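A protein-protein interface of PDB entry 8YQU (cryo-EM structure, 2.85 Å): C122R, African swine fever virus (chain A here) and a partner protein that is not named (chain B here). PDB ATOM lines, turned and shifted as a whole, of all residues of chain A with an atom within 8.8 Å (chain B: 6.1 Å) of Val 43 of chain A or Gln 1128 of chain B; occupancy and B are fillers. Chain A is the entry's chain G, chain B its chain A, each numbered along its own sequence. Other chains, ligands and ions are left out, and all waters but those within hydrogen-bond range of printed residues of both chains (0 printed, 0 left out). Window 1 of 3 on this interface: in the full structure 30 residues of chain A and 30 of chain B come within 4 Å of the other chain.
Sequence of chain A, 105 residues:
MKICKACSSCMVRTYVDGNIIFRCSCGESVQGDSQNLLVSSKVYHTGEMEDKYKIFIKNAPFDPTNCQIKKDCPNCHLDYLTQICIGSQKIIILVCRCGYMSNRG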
ATOM      1  N   SER A  40      -2.842  39.422  -6.500  1.00  0.00           N
ATOM      2  CA  SER A  40      -3.005  38.021  -6.861  1.00  0.00           C
ATOM      3  C   SER A  40      -3.130  37.197  -5.589  1.00  0.00           C
ATOM      4  O   SER A  40      -2.759  37.641  -4.500  1.00  0.00           O
ATOM      5  CB  SER A  40      -1.836  37.520  -7.715  1.00  0.00           C
ATOM      6  OG  SER A  40      -0.664  37.365  -6.934  1.00  0.00           O
ATOM      7  N   SER A  41      -3.659  35.987  -5.746  1.00  0.00           N
ATOM      8  CA  SER A  41      -3.809  35.073  -4.623  1.00  0.00           C
ATOM      9  C   SER A  41      -3.887  33.650  -5.152  1.00  0.00           C
ATOM     10  O   SER A  41      -4.218  33.418  -6.317  1.00  0.00           O
ATOM     11  CB  SER A  41      -5.052  35.406  -3.791  1.00  0.00           C
ATOM     12  OG  SER A  41      -6.236  35.183  -4.535  1.00  0.00           O
ATOM     13  N   LYS A  42      -3.575  32.700  -4.273  1.00  0.00           N
ATOM     14  CA  LYS A  42      -3.686  31.285  -4.596  1.00  0.00           C
ATOM     15  C   LYS A  42      -4.104  30.534  -3.342  1.00  0.00           C
ATOM     16  O   LYS A  42      -3.748  30.929  -2.229  1.00  0.00           O
ATOM     17  CB  LYS A  42      -2.368  30.722  -5.143  1.00  0.00           C
ATOM     18  CG  LYS A  42      -2.455  29.277  -5.610  1.00  0.00           C
ATOM     19  CD  LYS A  42      -1.150  28.799  -6.223  1.00  0.00           C
ATOM     20  CE  LYS A  42      -1.263  27.354  -6.684  1.00  0.00           C
ATOM     21  NZ  LYS A  42       0.001  26.853  -7.289  1.00  0.00           N
ATOM     22  N   VAL A  43      -4.863  29.458  -3.529  1.00  0.00           N
ATOM     23  CA  VAL A  43      -5.333  28.613  -2.439  1.00  0.00           C
ATOM     24  C   VAL A  43      -4.814  27.203  -2.676  1.00  0.00           C
ATOM     25  O   VAL A  43      -4.992  26.646  -3.765  1.00  0.00           O
ATOM     26  CB  VAL A  43      -6.869  28.624  -2.333  1.00  0.00           C
ATOM     27  CG1 VAL A  43      -7.354  27.468  -1.473  1.00  0.00           C
ATOM     28  CG2 VAL A  43      -7.348  29.952  -1.770  1.00  0.00           C
ATOM     29  N   TYR A  44      -4.169  26.634  -1.664  1.00  0.00           N
ATOM     30  CA  TYR A  44      -3.609  25.294  -1.743  1.00  0.00           C
ATOM     31  C   TYR A  44      -4.568  24.276  -1.140  1.00  0.00           C
ATOM     32  O   TYR A  44      -5.453  24.613  -0.348  1.00  0.00           O
ATOM     33  CB  TYR A  44      -2.256  25.231  -1.031  1.00  0.00           C
ATOM     34  CG  TYR A  44      -1.190  26.070  -1.693  1.00  0.00           C
ATOM     35  CD1 TYR A  44      -0.590  25.656  -2.873  1.00  0.00           C
ATOM     36  CD2 TYR A  44      -0.788  27.279  -1.144  1.00  0.00           C
ATOM     37  CE1 TYR A  44       0.382  26.418  -3.485  1.00  0.00           C
ATOM     38  CE2 TYR A  44       0.184  28.049  -1.748  1.00  0.00           C
ATOM     39  CZ  TYR A  44       0.765  27.614  -2.919  1.00  0.00           C
ATOM     40  OH  TYR A  44       1.734  28.375  -3.529  1.00  0.00           O
ATOM     41  N   HIS A  45      -4.375  23.014  -1.529  1.00  0.00           N
ATOM     42  CA  HIS A  45      -5.221  21.904  -1.089  1.00  0.00           C
ATOM     43  C   HIS A  45      -6.689  22.168  -1.423  1.00  0.00           C
ATOM     44  O   HIS A  45      -7.585  21.974  -0.599  1.00  0.00           O
ATOM     45  CB  HIS A  45      -5.038  21.628   0.406  1.00  0.00           C
ATOM     46  CG  HIS A  45      -3.609  21.449   0.816  1.00  0.00           C
ATOM     47  ND1 HIS A  45      -2.895  22.427   1.474  1.00  0.00           N
ATOM     48  CD2 HIS A  45      -2.759  20.407   0.657  1.00  0.00           C
ATOM     49  CE1 HIS A  45      -1.669  21.995   1.703  1.00  0.00           C
ATOM     50  NE2 HIS A  45      -1.560  20.772   1.218  1.00  0.00           N
ATOM     51  N   THR A  46      -6.929  22.622  -2.655  1.00  0.00           N
ATOM     52  CA  THR A  46      -8.291  22.880  -3.106  1.00  0.00           C
ATOM     53  C   THR A  46      -9.111  21.605  -3.242  1.00  0.00           C
ATOM     54  O   THR A  46     -10.344  21.677  -3.284  1.00  0.00           O
ATOM     55  CB  THR A  46      -8.277  23.623  -4.443  1.00  0.00           C
ATOM     56  OG1 THR A  46      -7.415  22.942  -5.363  1.00  0.00           O
ATOM     57  CG2 THR A  46      -7.788  25.049  -4.257  1.00  0.00           C
ATOM     58  N   GLY A  47      -8.462  20.446  -3.313  1.00  0.00           N
ATOM     59  CA  GLY A  47      -9.161  19.186  -3.450  1.00  0.00           C
ATOM     60  C   GLY A  47      -9.693  18.586  -2.171  1.00  0.00           C
ATOM     61  O   GLY A  47     -10.317  17.523  -2.214  1.00  0.00           O
ATOM     62  N   GLU A  48      -9.459  19.228  -1.022  1.00  0.00           N
ATOM     63  CA  GLU A  48      -9.979  18.709   0.238  1.00  0.00           C
ATOM     64  C   GLU A  48     -10.477  19.814   1.166  1.00  0.00           C
ATOM     65  O   GLU A  48     -10.602  19.582   2.375  1.00  0.00           O
ATOM     66  CB  GLU A  48      -8.920  17.866   0.954  1.00  0.00           C
ATOM     67  CG  GLU A  48      -7.676  18.634   1.369  1.00  0.00           C
ATOM     68  CD  GLU A  48      -6.611  17.732   1.961  1.00  0.00           C
ATOM     69  OE1 GLU A  48      -6.816  16.500   1.975  1.00  0.00           O
ATOM     70  OE2 GLU A  48      -5.571  18.254   2.414  1.00  0.00           O
ATOM     71  N   MET A  49     -10.767  21.002   0.642  1.00  0.00           N
ATOM     72  CA  MET A  49     -11.288  22.073   1.474  1.00  0.00           C
ATOM     73  C   MET A  49     -12.750  21.813   1.826  1.00  0.00           C
ATOM     74  O   MET A  49     -13.453  21.052   1.157  1.00  0.00           O
ATOM     75  CB  MET A  49     -11.143  23.425   0.772  1.00  0.00           C
ATOM     76  CG  MET A  49     -11.466  23.403  -0.711  1.00  0.00           C
ATOM     77  SD  MET A  49     -11.253  25.024  -1.474  1.00  0.00           S
ATOM     78  CE  MET A  49     -12.328  24.879  -2.898  1.00  0.00           C
ATOM     79  N   ASP A  51     -15.269  23.888   1.700  1.00  0.00           N
ATOM     80  CA  ASP A  51     -16.181  24.453   0.715  1.00  0.00           C
ATOM     81  C   ASP A  51     -16.352  23.563  -0.507  1.00  0.00           C
ATOM     82  O   ASP A  51     -17.346  23.710  -1.226  1.00  0.00           O
ATOM     83  CB  ASP A  51     -15.692  25.838   0.282  1.00  0.00           C
ATOM     84  CG  ASP A  51     -15.905  26.892   1.351  1.00  0.00           C
ATOM     85  OD1 ASP A  51     -16.922  26.813   2.071  1.00  0.00           O
ATOM     86  OD2 ASP A  51     -15.053  27.797   1.476  1.00  0.00           O
ATOM     87  N   ILE B1126       1.936  26.284   3.294  1.00  0.00           N
ATOM     88  CA  ILE B1126       1.023  27.397   3.067  1.00  0.00           C
ATOM     89  C   ILE B1126      -0.322  26.846   2.615  1.00  0.00           C
ATOM     90  O   ILE B1126      -0.381  25.996   1.719  1.00  0.00           O
ATOM     91  CB  ILE B1126       1.586  28.378   2.024  1.00  0.00           C
ATOM     92  CG1 ILE B1126       2.924  28.949   2.491  1.00  0.00           C
ATOM     93  CG2 ILE B1126       0.597  29.497   1.751  1.00  0.00           C
ATOM     94  CD1 ILE B1126       2.862  29.597   3.850  1.00  0.00           C
ATOM     95  N   LEU B1127      -1.397  27.326   3.240  1.00  0.00           N
ATOM     96  CA  LEU B1127      -2.737  27.014   2.755  1.00  0.00           C
ATOM     97  C   LEU B1127      -3.161  27.984   1.660  1.00  0.00           C
ATOM     98  O   LEU B1127      -3.733  27.576   0.642  1.00  0.00           O
ATOM     99  CB  LEU B1127      -3.739  27.041   3.909  1.00  0.00           C
ATOM    100  CG  LEU B1127      -4.151  25.708   4.531  1.00  0.00           C
ATOM    101  CD1 LEU B1127      -5.179  25.935   5.624  1.00  0.00           C
ATOM    102  CD2 LEU B1127      -4.692  24.766   3.469  1.00  0.00           C
ATOM    103  N   GLN B1128      -2.895  29.273   1.854  1.00  0.00           N
ATOM    104  CA  GLN B1128      -3.210  30.283   0.856  1.00  0.00           C
ATOM    105  C   GLN B1128      -2.315  31.492   1.082  1.00  0.00           C
ATOM    106  O   GLN B1128      -1.896  31.766   2.209  1.00  0.00           O
ATOM    107  CB  GLN B1128      -4.687  30.691   0.916  1.00  0.00           C
ATOM    108  CG  GLN B1128      -5.121  31.252   2.257  1.00  0.00           C
ATOM    109  CD  GLN B1128      -6.626  31.330   2.394  1.00  0.00           C
ATOM    110  OE1 GLN B1128      -7.361  31.044   1.451  1.00  0.00           O
ATOM    111  NE2 GLN B1128      -7.093  31.718   3.574  1.00  0.00           N
ATOM    112  N   TRP B1129      -2.025  32.210  -0.003  1.00  0.00           N
ATOM    113  CA  TRP B1129      -1.213  33.414   0.065  1.00  0.00           C
ATOM    114  C   TRP B1129      -1.871  34.530  -0.732  1.00  0.00           C
ATOM    115  O   TRP B1129      -2.533  34.287  -1.744  1.00  0.00           O
ATOM    116  CB  TRP B1129       0.215  33.173  -0.446  1.00  0.00           C
ATOM    117  CG  TRP B1129       0.323  32.718  -1.865  1.00  0.00           C
ATOM    118  CD1 TRP B1129       0.417  31.433  -2.307  1.00  0.00           C
ATOM    119  CD2 TRP B1129       0.390  33.549  -3.030  1.00  0.00           C
ATOM    120  NE1 TRP B1129       0.520  31.409  -3.676  1.00  0.00           N
ATOM    121  CE2 TRP B1129       0.506  32.696  -4.144  1.00  0.00           C
ATOM    122  CE3 TRP B1129       0.354  34.931  -3.239  1.00  0.00           C
ATOM    123  CZ2 TRP B1129       0.585  33.179  -5.448  1.00  0.00           C
ATOM    124  CZ3 TRP B1129       0.433  35.408  -4.533  1.00  0.00           C
ATOM    125  CH2 TRP B1129       0.548  34.535  -5.621  1.00  0.00           C
ATOM    126  N   HIS B1130      -1.680  35.760  -0.260  1.00  0.00           N
ATOM    127  CA  HIS B1130      -2.256  36.945  -0.877  1.00  0.00           C
ATOM    128  C   HIS B1130      -1.167  37.982  -1.107  1.00  0.00           C
ATOM    129  O   HIS B1130      -0.364  38.259  -0.212  1.00  0.00           O
ATOM    130  CB  HIS B1130      -3.366  37.541  -0.002  1.00  0.00           C
ATOM    131  CG  HIS B1130      -4.564  36.657   0.144  1.00  0.00           C
ATOM    132  ND1 HIS B1130      -5.598  36.649  -0.766  1.00  0.00           N
ATOM    133  CD2 HIS B1130      -4.890  35.748   1.093  1.00  0.00           C
ATOM    134  CE1 HIS B1130      -6.512  35.775  -0.383  1.00  0.00           C
ATOM    135  NE2 HIS B1130      -6.107  35.215   0.742  1.00  0.00           N
ATOM    136  N   ARG B1177       0.770  38.246   2.134  1.00  0.00           N
ATOM    137  CA  ARG B1177       0.092  37.725   3.311  1.00  0.00           C
ATOM    138  C   ARG B1177       0.002  36.210   3.208  1.00  0.00           C
ATOM    139  O   ARG B1177      -0.400  35.675   2.170  1.00  0.00           O
ATOM    140  CB  ARG B1177      -1.302  38.331   3.466  1.00  0.00           C
ATOM    141  CG  ARG B1177      -1.946  38.025   4.808  1.00  0.00           C
ATOM    142  CD  ARG B1177      -3.347  38.592   4.893  1.00  0.00           C
ATOM    143  NE  ARG B1177      -3.934  38.407   6.215  1.00  0.00           N
ATOM    144  CZ  ARG B1177      -4.551  37.303   6.611  1.00  0.00           C
ATOM    145  NH1 ARG B1177      -4.678  36.258   5.810  1.00  0.00           N
ATOM    146  NH2 ARG B1177      -5.056  37.248   7.840  1.00  0.00           N
ATOM    147  N   LEU B1178       0.374  35.529   4.286  1.00  0.00           N
ATOM    148  CA  LEU B1178       0.506  34.081   4.308  1.00  0.00           C
ATOM    149  C   LEU B1178      -0.324  33.518   5.449  1.00  0.00           C
ATOM    150  O   LEU B1178      -0.344  34.082   6.547  1.00  0.00           O
ATOM    151  CB  LEU B1178       1.974  33.693   4.479  1.00  0.00           C
ATOM    152  CG  LEU B1178       2.889  34.103   3.327  1.00  0.00           C
ATOM    153  CD1 LEU B1178       4.327  33.859   3.691  1.00  0.00           C
ATOM    154  CD2 LEU B1178       2.541  33.323   2.086  1.00  0.00           C
ATOM    155  N   GLU B1179      -1.009  32.408   5.192  1.00  0.00           N
ATOM    156  CA  GLU B1179      -1.817  31.734   6.203  1.00  0.00           C
ATOM    157  C   GLU B1179      -1.318  30.298   6.295  1.00  0.00           C
ATOM    158  O   GLU B1179      -1.622  29.472   5.427  1.00  0.00           O
ATOM    159  CB  GLU B1179      -3.305  31.807   5.856  1.00  0.00           C
ATOM    160  CG  GLU B1179      -4.251  31.381   6.973  1.00  0.00           C
ATOM    161  CD  GLU B1179      -4.479  29.886   7.025  1.00  0.00           C
ATOM    162  OE1 GLU B1179      -4.391  29.237   5.966  1.00  0.00           O
ATOM    163  OE2 GLU B1179      -4.755  29.358   8.123  1.00  0.00           O
ATOM    164  N   LEU B1180      -0.545  30.010   7.340  1.00  0.00           N
ATOM    165  CA  LEU B1180       0.138  28.728   7.449  1.00  0.00           C
ATOM    166  C   LEU B1180      -0.849  27.590   7.673  1.00  0.00           C
ATOM    167  O   LEU B1180      -1.869  27.749   8.347  1.00  0.00           O
ATOM    168  CB  LEU B1180       1.150  28.767   8.592  1.00  0.00           C
ATOM    169  CG  LEU B1180       2.496  29.437   8.312  1.00  0.00           C
ATOM    170  CD1 LEU B1180       3.271  29.619   9.600  1.00  0.00           C
ATOM    171  CD2 LEU B1180       3.302  28.618   7.321  1.00  0.00           C
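O of Leu 1127 of chain B lies within hydrogen-bond range of N of Tyr 44 of chain A (2.5 Å).
N of Trp 1129 of chain B sits at hydrogen-bond distance from O of Lys 42 of chain A (3.1 Å).
NE1 of Trp 1129 of chain B is in hydrogen-bond range of OH of Tyr 44 of chain A, at 3.3 Å.
The backbone carbonyl oxygen (O) of Glu 1179 of chain B sits at hydrogen-bond distance from the backbone NH (N) of Leu 1127 of chain B (3.1 Å).
The backbone carbonyl oxygen of Gln 1128 of chain B lies within hydrogen-bond range of the backbone NH of Glu 1179 of chain B.
O of His 1130 of chain B sits at hydrogen-bond distance from N of Arg 1177 of chain B, 2.6 Å away.
Among the printed residues, pairs that only touch across the chains: Tyr 44 of chain A with Ile 1126 of chain B (3.2 Å), Lys 42 of chain A with Gln 1128 of chain B (3.2 Å), Ser 41 of chain A with Trp 1129 of chain B (3.2 Å), Ser 40 of chain A with Trp 1129 of chain B (3.3 Å), Ser 41 of chain A with His 1130 of chain B (3.3 Å), Val 43 of chain A with Gln 1128 of chain B (3.4 Å), Val 43 of chain A with Leu 1127 of chain B (3.5 Å), His 45 of chain A with Leu 1127 of chain B (3.6 Å) and Ser 40 of chain A with His 1130 of chain B (3.7 Å).
Of chain B, only Leu 1127 (3.5 Å) and Gln 1128 (3.4 Å) come within 4 Å of Val 43 of chain A.
Of the printed residues of chain B, His 45 of chain A touches Leu 1127 (3.6 Å).
Of the printed residues of chain A, Ile 1126 of chain B touches Tyr 44.
Of the printed residues of chain A, Leu 1127 of chain B touches Val 43 (3.5 Å), Tyr 44 (2.5 Å) and His 45 (3.6 Å).
Printed residues of chain A within 4 Å of Trp 1129 of chain B: Ser 40, Ser 41, Lys 42 and Tyr 44.
Printed residues of chain A within 4 Å of His 1130 of chain B: Ser 40 and Ser 41.
The nearest residue of chain A that does not touch Gln 1128 of chain B is Tyr 44 of chain A (4.2 Å).
The nearest printed residue of chain B that does not touch His 45 of chain A is Ile 1126 of chain B (4.2 Å).
Of the 9 printed residues of chain B, 5 touch a printed residue of chain A.
Hydrophobic or aromatic side chains of chain B within 4 Å of the printed part of chain A: Ile 1126, Leu 1127, Trp 1129 and His 1130.
Of the 11 printed residues of chain A, 6 touch a printed residue of chain B.
Hydrophobic or aromatic side chains of chain A within 4 Å of the printed part of chain B: Val 43, Tyr 44 and His 45.
Among the printed residues, 12 pairs touch across the chains.
Among the printed residues, no Asp or Glu carboxylate lies within 4 Å of a Lys or Arg side-chain nitrogen of the other chain.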
